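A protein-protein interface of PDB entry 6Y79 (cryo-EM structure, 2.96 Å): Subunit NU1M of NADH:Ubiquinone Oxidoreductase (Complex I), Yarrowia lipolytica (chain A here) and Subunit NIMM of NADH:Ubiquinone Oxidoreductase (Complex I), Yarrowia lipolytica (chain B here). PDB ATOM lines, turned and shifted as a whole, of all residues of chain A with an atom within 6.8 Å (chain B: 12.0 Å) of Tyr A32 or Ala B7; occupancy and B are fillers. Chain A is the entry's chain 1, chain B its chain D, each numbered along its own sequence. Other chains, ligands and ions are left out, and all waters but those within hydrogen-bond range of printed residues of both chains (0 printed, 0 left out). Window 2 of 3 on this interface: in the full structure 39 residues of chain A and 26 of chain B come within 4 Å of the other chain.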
ATOM      1  N   VAL A  24      34.586 -30.922   9.775  1.00  0.00           N
ATOM      2  CA  VAL A  24      34.324 -30.271  11.073  1.00  0.00           C
ATOM      3  C   VAL A  24      33.359 -29.098  10.906  1.00  0.00           C
ATOM      4  O   VAL A  24      32.395 -28.954  11.675  1.00  0.00           O
ATOM      5  CB  VAL A  24      35.635 -29.833  11.755  1.00  0.00           C
ATOM      6  CG1 VAL A  24      35.375 -29.295  13.143  1.00  0.00           C
ATOM      7  CG2 VAL A  24      36.626 -31.006  11.864  1.00  0.00           C
ATOM      8  N   ALA A  25      33.498 -28.367   9.793  1.00  0.00           N
ATOM      9  CA  ALA A  25      32.596 -27.260   9.480  1.00  0.00           C
ATOM     10  C   ALA A  25      31.160 -27.716   9.187  1.00  0.00           C
ATOM     11  O   ALA A  25      30.202 -27.029   9.576  1.00  0.00           O
ATOM     12  CB  ALA A  25      33.148 -26.446   8.306  1.00  0.00           C
ATOM     13  N   GLU A  26      30.973 -28.836   8.475  1.00  0.00           N
ATOM     14  CA  GLU A  26      29.597 -29.263   8.211  1.00  0.00           C
ATOM     15  C   GLU A  26      28.911 -29.731   9.470  1.00  0.00           C
ATOM     16  O   GLU A  26      27.718 -29.474   9.644  1.00  0.00           O
ATOM     17  CB  GLU A  26      29.472 -30.320   7.113  1.00  0.00           C
ATOM     18  CG  GLU A  26      30.245 -31.580   7.201  1.00  0.00           C
ATOM     19  CD  GLU A  26      29.644 -32.607   8.078  1.00  0.00           C
ATOM     20  OE1 GLU A  26      28.395 -32.699   8.289  1.00  0.00           O
ATOM     21  OE2 GLU A  26      30.476 -33.323   8.691  1.00  0.00           O
ATOM     22  N   ARG A  27      29.638 -30.404  10.366  1.00  0.00           N
ATOM     23  CA  ARG A  27      28.961 -30.816  11.600  1.00  0.00           C
ATOM     24  C   ARG A  27      28.572 -29.621  12.438  1.00  0.00           C
ATOM     25  O   ARG A  27      27.457 -29.568  12.973  1.00  0.00           O
ATOM     26  CB  ARG A  27      29.790 -31.787  12.440  1.00  0.00           C
ATOM     27  CG  ARG A  27      29.735 -33.134  11.840  1.00  0.00           C
ATOM     28  CD  ARG A  27      30.702 -34.096  12.451  1.00  0.00           C
ATOM     29  NE  ARG A  27      30.381 -34.543  13.798  1.00  0.00           N
ATOM     30  CZ  ARG A  27      31.122 -35.432  14.441  1.00  0.00           C
ATOM     31  NH1 ARG A  27      32.191 -35.905  13.828  1.00  0.00           N
ATOM     32  NH2 ARG A  27      30.816 -35.855  15.671  1.00  0.00           N
ATOM     33  N   LYS A  28      29.439 -28.623  12.511  1.00  0.00           N
ATOM     34  CA  LYS A  28      29.115 -27.481  13.353  1.00  0.00           C
ATOM     35  C   LYS A  28      27.971 -26.641  12.782  1.00  0.00           C
ATOM     36  O   LYS A  28      27.038 -26.300  13.512  1.00  0.00           O
ATOM     37  CB  LYS A  28      30.364 -26.650  13.601  1.00  0.00           C
ATOM     38  CG  LYS A  28      31.366 -27.484  14.374  1.00  0.00           C
ATOM     39  CD  LYS A  28      32.521 -26.690  14.861  1.00  0.00           C
ATOM     40  CE  LYS A  28      32.056 -25.775  15.955  1.00  0.00           C
ATOM     41  NZ  LYS A  28      31.731 -26.445  17.229  1.00  0.00           N
ATOM     42  N   THR A  29      27.950 -26.376  11.467  1.00  0.00           N
ATOM     43  CA  THR A  29      26.838 -25.541  10.985  1.00  0.00           C
ATOM     44  C   THR A  29      25.540 -26.316  10.817  1.00  0.00           C
ATOM     45  O   THR A  29      24.457 -25.718  10.911  1.00  0.00           O
ATOM     46  CB  THR A  29      27.186 -24.837   9.688  1.00  0.00           C
ATOM     47  OG1 THR A  29      27.274 -25.793   8.630  1.00  0.00           O
ATOM     48  CG2 THR A  29      28.474 -24.171   9.882  1.00  0.00           C
ATOM     49  N   LEU A  30      25.611 -27.632  10.588  1.00  0.00           N
ATOM     50  CA  LEU A  30      24.402 -28.438  10.680  1.00  0.00           C
ATOM     51  C   LEU A  30      23.854 -28.421  12.096  1.00  0.00           C
ATOM     52  O   LEU A  30      22.637 -28.386  12.291  1.00  0.00           O
ATOM     53  CB  LEU A  30      24.675 -29.873  10.235  1.00  0.00           C
ATOM     54  CG  LEU A  30      24.647 -30.166   8.737  1.00  0.00           C
ATOM     55  CD1 LEU A  30      24.965 -31.627   8.470  1.00  0.00           C
ATOM     56  CD2 LEU A  30      23.315 -29.787   8.160  1.00  0.00           C
ATOM     57  N   ALA A  31      24.739 -28.380  13.095  1.00  0.00           N
ATOM     58  CA  ALA A  31      24.290 -28.306  14.478  1.00  0.00           C
ATOM     59  C   ALA A  31      23.635 -26.967  14.791  1.00  0.00           C
ATOM     60  O   ALA A  31      22.578 -26.918  15.426  1.00  0.00           O
ATOM     61  CB  ALA A  31      25.467 -28.543  15.405  1.00  0.00           C
ATOM     62  N   TYR A  32      24.259 -25.866  14.369  1.00  0.00           N
ATOM     63  CA  TYR A  32      23.709 -24.554  14.711  1.00  0.00           C
ATOM     64  C   TYR A  32      22.452 -24.231  13.913  1.00  0.00           C
ATOM     65  O   TYR A  32      21.619 -23.447  14.377  1.00  0.00           O
ATOM     66  CB  TYR A  32      24.755 -23.460  14.519  1.00  0.00           C
ATOM     67  CG  TYR A  32      25.771 -23.401  15.631  1.00  0.00           C
ATOM     68  CD1 TYR A  32      25.493 -22.767  16.829  1.00  0.00           C
ATOM     69  CD2 TYR A  32      27.005 -23.984  15.482  1.00  0.00           C
ATOM     70  CE1 TYR A  32      26.430 -22.727  17.839  1.00  0.00           C
ATOM     71  CE2 TYR A  32      27.941 -23.954  16.471  1.00  0.00           C
ATOM     72  CZ  TYR A  32      27.655 -23.327  17.649  1.00  0.00           C
ATOM     73  OH  TYR A  32      28.609 -23.304  18.634  1.00  0.00           O
ATOM     74  N   MET A  33      22.296 -24.819  12.724  1.00  0.00           N
ATOM     75  CA  MET A  33      21.023 -24.710  12.020  1.00  0.00           C
ATOM     76  C   MET A  33      19.924 -25.458  12.760  1.00  0.00           C
ATOM     77  O   MET A  33      18.751 -25.083  12.683  1.00  0.00           O
ATOM     78  CB  MET A  33      21.163 -25.237  10.594  1.00  0.00           C
ATOM     79  CG  MET A  33      21.814 -24.270   9.628  1.00  0.00           C
ATOM     80  SD  MET A  33      22.512 -25.102   8.194  1.00  0.00           S
ATOM     81  CE  MET A  33      23.561 -23.813   7.544  1.00  0.00           C
ATOM     82  N   GLN A  34      20.293 -26.520  13.478  1.00  0.00           N
ATOM     83  CA  GLN A  34      19.381 -27.322  14.278  1.00  0.00           C
ATOM     84  C   GLN A  34      19.375 -26.921  15.740  1.00  0.00           C
ATOM     85  O   GLN A  34      18.852 -27.669  16.569  1.00  0.00           O
ATOM     86  CB  GLN A  34      19.738 -28.793  14.128  1.00  0.00           C
ATOM     87  CG  GLN A  34      19.565 -29.222  12.693  1.00  0.00           C
ATOM     88  CD  GLN A  34      20.061 -30.610  12.402  1.00  0.00           C
ATOM     89  OE1 GLN A  34      20.744 -31.247  13.192  1.00  0.00           O
ATOM     90  NE2 GLN A  34      19.688 -31.100  11.222  1.00  0.00           N
ATOM     91  N   ARG A  35      19.961 -25.763  16.056  1.00  0.00           N
ATOM     92  CA  ARG A  35      19.935 -25.130  17.375  1.00  0.00           C
ATOM     93  C   ARG A  35      20.565 -26.006  18.450  1.00  0.00           C
ATOM     94  O   ARG A  35      20.023 -26.185  19.539  1.00  0.00           O
ATOM     95  CB  ARG A  35      18.522 -24.724  17.758  1.00  0.00           C
ATOM     96  CG  ARG A  35      17.922 -23.785  16.770  1.00  0.00           C
ATOM     97  CD  ARG A  35      16.517 -23.517  17.146  1.00  0.00           C
ATOM     98  NE  ARG A  35      16.453 -22.949  18.479  1.00  0.00           N
ATOM     99  CZ  ARG A  35      16.604 -21.668  18.770  1.00  0.00           C
ATOM    100  NH1 ARG A  35      16.804 -20.816  17.797  1.00  0.00           N
ATOM    101  NH2 ARG A  35      16.529 -21.242  20.022  1.00  0.00           N
ATOM    102  N   ARG A  36      21.736 -26.536  18.138  1.00  0.00           N
ATOM    103  CA  ARG A  36      22.544 -27.227  19.121  1.00  0.00           C
ATOM    104  C   ARG A  36      23.995 -26.901  18.832  1.00  0.00           C
ATOM    105  O   ARG A  36      24.331 -26.336  17.792  1.00  0.00           O
ATOM    106  CB  ARG A  36      22.294 -28.730  19.094  1.00  0.00           C
ATOM    107  CG  ARG A  36      22.239 -29.308  17.710  1.00  0.00           C
ATOM    108  CD  ARG A  36      22.337 -30.799  17.769  1.00  0.00           C
ATOM    109  NE  ARG A  36      22.478 -31.401  16.450  1.00  0.00           N
ATOM    110  CZ  ARG A  36      23.644 -31.759  15.942  1.00  0.00           C
ATOM    111  NH1 ARG A  36      24.737 -31.572  16.658  1.00  0.00           N
ATOM    112  NH2 ARG A  36      23.724 -32.301  14.738  1.00  0.00           N
ATOM    113  N   LEU A  37      24.855 -27.240  19.775  1.00  0.00           N
ATOM    114  CA  LEU A  37      26.266 -27.046  19.537  1.00  0.00           C
ATOM    115  C   LEU A  37      26.797 -28.137  18.625  1.00  0.00           C
ATOM    116  O   LEU A  37      26.272 -29.248  18.565  1.00  0.00           O
ATOM    117  CB  LEU A  37      27.040 -27.049  20.848  1.00  0.00           C
ATOM    118  CG  LEU A  37      27.380 -25.672  21.395  1.00  0.00           C
ATOM    119  CD1 LEU A  37      26.174 -25.021  22.002  1.00  0.00           C
ATOM    120  CD2 LEU A  37      28.459 -25.816  22.408  1.00  0.00           C
ATOM    121  N   GLY A  38      27.858 -27.816  17.907  1.00  0.00           N
ATOM    122  CA  GLY A  38      28.611 -28.834  17.224  1.00  0.00           C
ATOM    123  C   GLY A  38      29.534 -29.526  18.197  1.00  0.00           C
ATOM    124  O   GLY A  38      29.393 -29.403  19.416  1.00  0.00           O
ATOM    125  N   ALA B   2      24.214 -14.322  18.638  1.00  0.00           N
ATOM    126  CA  ALA B   2      23.830 -14.244  17.236  1.00  0.00           C
ATOM    127  C   ALA B   2      24.663 -15.169  16.380  1.00  0.00           C
ATOM    128  O   ALA B   2      24.413 -16.373  16.339  1.00  0.00           O
ATOM    129  CB  ALA B   2      23.966 -12.862  16.746  1.00  0.00           C
ATOM    130  N   ILE B   3      25.640 -14.582  15.691  1.00  0.00           N
ATOM    131  CA  ILE B   3      26.544 -15.345  14.832  1.00  0.00           C
ATOM    132  C   ILE B   3      27.383 -16.270  15.695  1.00  0.00           C
ATOM    133  O   ILE B   3      28.114 -15.791  16.585  1.00  0.00           O
ATOM    134  CB  ILE B   3      27.447 -14.403  14.020  1.00  0.00           C
ATOM    135  CG1 ILE B   3      26.625 -13.525  13.094  1.00  0.00           C
ATOM    136  CG2 ILE B   3      28.448 -15.181  13.221  1.00  0.00           C
ATOM    137  CD1 ILE B   3      26.642 -12.100  13.492  1.00  0.00           C
ATOM    138  N   PRO B   4      27.305 -17.577  15.506  1.00  0.00           N
ATOM    139  CA  PRO B   4      28.210 -18.465  16.234  1.00  0.00           C
ATOM    140  C   PRO B   4      29.618 -18.331  15.694  1.00  0.00           C
ATOM    141  O   PRO B   4      29.853 -18.542  14.502  1.00  0.00           O
ATOM    142  CB  PRO B   4      27.622 -19.856  15.983  1.00  0.00           C
ATOM    143  CG  PRO B   4      26.825 -19.725  14.744  1.00  0.00           C
ATOM    144  CD  PRO B   4      26.383 -18.310  14.621  1.00  0.00           C
ATOM    145  N   PHE B   5      30.557 -17.938  16.548  1.00  0.00           N
ATOM    146  CA  PHE B   5      31.938 -17.884  16.099  1.00  0.00           C
ATOM    147  C   PHE B   5      32.494 -19.279  15.881  1.00  0.00           C
ATOM    148  O   PHE B   5      33.267 -19.487  14.940  1.00  0.00           O
ATOM    149  CB  PHE B   5      32.802 -17.091  17.086  1.00  0.00           C
ATOM    150  CG  PHE B   5      32.904 -17.692  18.466  1.00  0.00           C
ATOM    151  CD1 PHE B   5      31.914 -17.471  19.415  1.00  0.00           C
ATOM    152  CD2 PHE B   5      34.019 -18.430  18.829  1.00  0.00           C
ATOM    153  CE1 PHE B   5      32.016 -18.006  20.677  1.00  0.00           C
ATOM    154  CE2 PHE B   5      34.129 -18.964  20.096  1.00  0.00           C
ATOM    155  CZ  PHE B   5      33.127 -18.751  21.020  1.00  0.00           C
ATOM    156  N   GLU B   6      32.059 -20.248  16.693  1.00  0.00           N
ATOM    157  CA  GLU B   6      32.567 -21.611  16.593  1.00  0.00           C
ATOM    158  C   GLU B   6      32.196 -22.269  15.278  1.00  0.00           C
ATOM    159  O   GLU B   6      33.016 -23.000  14.724  1.00  0.00           O
ATOM    160  CB  GLU B   6      32.051 -22.469  17.741  1.00  0.00           C
ATOM    161  CG  GLU B   6      32.624 -22.113  19.073  1.00  0.00           C
ATOM    162  CD  GLU B   6      32.101 -23.009  20.158  1.00  0.00           C
ATOM    163  OE1 GLU B   6      31.228 -23.851  19.861  1.00  0.00           O
ATOM    164  OE2 GLU B   6      32.556 -22.867  21.309  1.00  0.00           O
ATOM    165  N   ALA B   7      30.995 -22.004  14.757  1.00  0.00           N
ATOM    166  CA  ALA B   7      30.584 -22.580  13.480  1.00  0.00           C
ATOM    167  C   ALA B   7      31.450 -22.077  12.336  1.00  0.00           C
ATOM    168  O   ALA B   7      31.778 -22.829  11.414  1.00  0.00           O
ATOM    169  CB  ALA B   7      29.119 -22.254  13.202  1.00  0.00           C
ATOM    170  N   LEU B   8      31.836 -20.807  12.385  1.00  0.00           N
ATOM    171  CA  LEU B   8      32.587 -20.190  11.304  1.00  0.00           C
ATOM    172  C   LEU B   8      34.085 -20.225  11.517  1.00  0.00           C
ATOM    173  O   LEU B   8      34.822 -19.719  10.664  1.00  0.00           O
ATOM    174  CB  LEU B   8      32.164 -18.745  11.126  1.00  0.00           C
ATOM    175  CG  LEU B   8      30.709 -18.566  10.767  1.00  0.00           C
ATOM    176  CD1 LEU B   8      30.440 -17.104  10.820  1.00  0.00           C
ATOM    177  CD2 LEU B   8      30.435 -19.126   9.381  1.00  0.00           C
ATOM    178  N   LEU B   9      34.554 -20.758  12.634  1.00  0.00           N
ATOM    179  CA  LEU B   9      35.996 -20.920  12.739  1.00  0.00           C
ATOM    180  C   LEU B   9      36.578 -21.991  11.808  1.00  0.00           C
ATOM    181  O   LEU B   9      37.591 -21.674  11.180  1.00  0.00           O
ATOM    182  CB  LEU B   9      36.418 -21.124  14.197  1.00  0.00           C
ATOM    183  CG  LEU B   9      36.529 -19.728  14.825  1.00  0.00           C
ATOM    184  CD1 LEU B   9      36.722 -19.771  16.351  1.00  0.00           C
ATOM    185  CD2 LEU B   9      37.550 -18.692  14.084  1.00  0.00           C
ATOM    186  N   PRO B  10      36.015 -23.209  11.629  1.00  0.00           N
ATOM    187  CA  PRO B  10      36.601 -24.122  10.625  1.00  0.00           C
ATOM    188  C   PRO B  10      36.518 -23.609   9.204  1.00  0.00           C
ATOM    189  O   PRO B  10      37.414 -23.904   8.403  1.00  0.00           O
ATOM    190  CB  PRO B  10      35.782 -25.404  10.796  1.00  0.00           C
ATOM    191  CG  PRO B  10      35.267 -25.335  12.135  1.00  0.00           C
ATOM    192  CD  PRO B  10      34.966 -23.922  12.381  1.00  0.00           C
ATOM    193  N   TYR B  11      35.496 -22.816   8.882  1.00  0.00           N
ATOM    194  CA  TYR B  11      35.524 -22.024   7.660  1.00  0.00           C
ATOM    195  C   TYR B  11      36.650 -21.011   7.684  1.00  0.00           C
ATOM    196  O   TYR B  11      37.244 -20.723   6.644  1.00  0.00           O
ATOM    197  CB  TYR B  11      34.206 -21.295   7.469  1.00  0.00           C
ATOM    198  CG  TYR B  11      33.081 -22.214   7.181  1.00  0.00           C
ATOM    199  CD1 TYR B  11      32.894 -22.730   5.907  1.00  0.00           C
ATOM    200  CD2 TYR B  11      32.213 -22.578   8.174  1.00  0.00           C
ATOM    201  CE1 TYR B  11      31.857 -23.584   5.642  1.00  0.00           C
ATOM    202  CE2 TYR B  11      31.193 -23.415   7.919  1.00  0.00           C
ATOM    203  CZ  TYR B  11      31.008 -23.919   6.661  1.00  0.00           C
ATOM    204  OH  TYR B  11      29.962 -24.763   6.435  1.00  0.00           O
ATOM    205  N   GLY B  12      36.944 -20.450   8.858  1.00  0.00           N
ATOM    206  CA  GLY B  12      38.053 -19.522   8.967  1.00  0.00           C
ATOM    207  C   GLY B  12      39.389 -20.178   8.693  1.00  0.00           C
ATOM    208  O   GLY B  12      40.260 -19.587   8.057  1.00  0.00           O
ATOM    209  N   ILE B  13      39.551 -21.428   9.123  1.00  0.00           N
ATOM    210  CA  ILE B  13      40.807 -22.122   8.869  1.00  0.00           C
ATOM    211  C   ILE B  13      40.871 -22.595   7.419  1.00  0.00           C
ATOM    212  O   ILE B  13      41.936 -22.546   6.802  1.00  0.00           O
ATOM    213  CB  ILE B  13      41.042 -23.254   9.894  1.00  0.00           C
ATOM    214  CG1 ILE B  13      41.401 -22.694  11.276  1.00  0.00           C
ATOM    215  CG2 ILE B  13      42.188 -24.165   9.510  1.00  0.00           C
ATOM    216  CD1 ILE B  13      40.357 -22.848  12.334  1.00  0.00           C
ATOM    217  N   ILE B  14      39.733 -23.001   6.833  1.00  0.00           N
ATOM    218  CA  ILE B  14      39.695 -23.318   5.397  1.00  0.00           C
ATOM    219  C   ILE B  14      40.086 -22.100   4.561  1.00  0.00           C
ATOM    220  O   ILE B  14      40.940 -22.182   3.660  1.00  0.00           O
ATOM    221  CB  ILE B  14      38.300 -23.838   4.997  1.00  0.00           C
ATOM    222  CG1 ILE B  14      38.058 -25.242   5.530  1.00  0.00           C
ATOM    223  CG2 ILE B  14      38.144 -23.881   3.494  1.00  0.00           C
ATOM    224  CD1 ILE B  14      36.597 -25.613   5.534  1.00  0.00           C
ATOM    225  N   PHE B  15      39.512 -20.945   4.901  1.00  0.00           N
ATOM    226  CA  PHE B  15      39.818 -19.680   4.247  1.00  0.00           C
ATOM    227  C   PHE B  15      41.284 -19.300   4.417  1.00  0.00           C
ATOM    228  O   PHE B  15      41.949 -18.904   3.455  1.00  0.00           O
ATOM    229  CB  PHE B  15      38.901 -18.607   4.831  1.00  0.00           C
ATOM    230  CG  PHE B  15      39.125 -17.241   4.286  1.00  0.00           C
ATOM    231  CD1 PHE B  15      38.644 -16.900   3.041  1.00  0.00           C
ATOM    232  CD2 PHE B  15      39.789 -16.286   5.032  1.00  0.00           C
ATOM    233  CE1 PHE B  15      38.836 -15.637   2.539  1.00  0.00           C
ATOM    234  CE2 PHE B  15      39.988 -15.020   4.534  1.00  0.00           C
ATOM    235  CZ  PHE B  15      39.511 -14.696   3.287  1.00  0.00           C
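The side-chain hydroxyl (OG1) of Thr A29 is in hydrogen-bond range of the backbone carbonyl oxygen (O) of Ala A25, 3.3 Å away.
NZ of Lys A28 is in salt-bridge range of OE1 of Glu B6.
The side-chain hydroxyl (OH) of Tyr A32 lies within hydrogen-bond range of the side-chain carboxylate (OE1) of Glu B6 (2.9 Å).
Of chain B, only Pro B10 (3.8 Å) and Tyr B11 (3.6 Å) come within 4 Å of Ala A25.
Of chain B, only Glu B6 comes within 4 Å of Lys A28.
Thr A29 touches two residues of chain B.
No residue of chain B comes within 4 Å of Ala A31.
Of chain B, only Pro B4 (3.6 Å), Glu B6 (2.9 Å) and Ala B7 (3.6 Å) come within 4 Å of Tyr A32.
No residue of chain B comes within 4 Å of Gln A34.
No residue of chain B comes within 4 Å of Arg A35.
Arg A36 touches none of the printed residues of chain B.
No residue of chain B comes within 4 Å of Leu A37.
No residue of chain B comes within 4 Å of Gly A38.
Of the printed residues of chain A, Pro B4 touches Tyr A32 (3.6 Å).
Printed residues of chain A within 4 Å of Glu B6: Lys A28 and Tyr A32.
Of chain A, only Thr A29 (3.9 Å) and Tyr A32 (3.6 Å) come within 4 Å of Ala B7.
Of the printed residues of chain A, Pro B10 touches Ala A25 (3.8 Å).
Printed residues of chain A within 4 Å of Tyr B11: Ala A25 and Thr A29.
The nearest residue of chain A that does not touch Ala B7 is Lys A28 (4.1 Å).
The nearest printed residue of chain A that does not touch Glu B6 is Leu A37 (4.2 Å).
Ala A25 touches Pro B10.
CB of Ala A25 touches CE2 of Tyr B11 (3.6 Å).
Thr A29 touches Ala B7.
CE2 of Tyr B11 touches CG2 of Thr A29, 3.4 Å away.
CE1 of Tyr A32 touches CB of Pro B4, at 3.6 Å.
Tyr A32 touches Ala B7.
Hydrophobic or aromatic side chains of chain B within 4 Å of the printed part of chain A: Pro B4, Ala B7, Pro B10 and Tyr B11.
Hydrophobic or aromatic side chains of chain A that line the printed part of chain B: Ala A25 and Tyr A32.
Along chain A the printed residues that touch a printed residue of chain B span positions 25 to 32.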
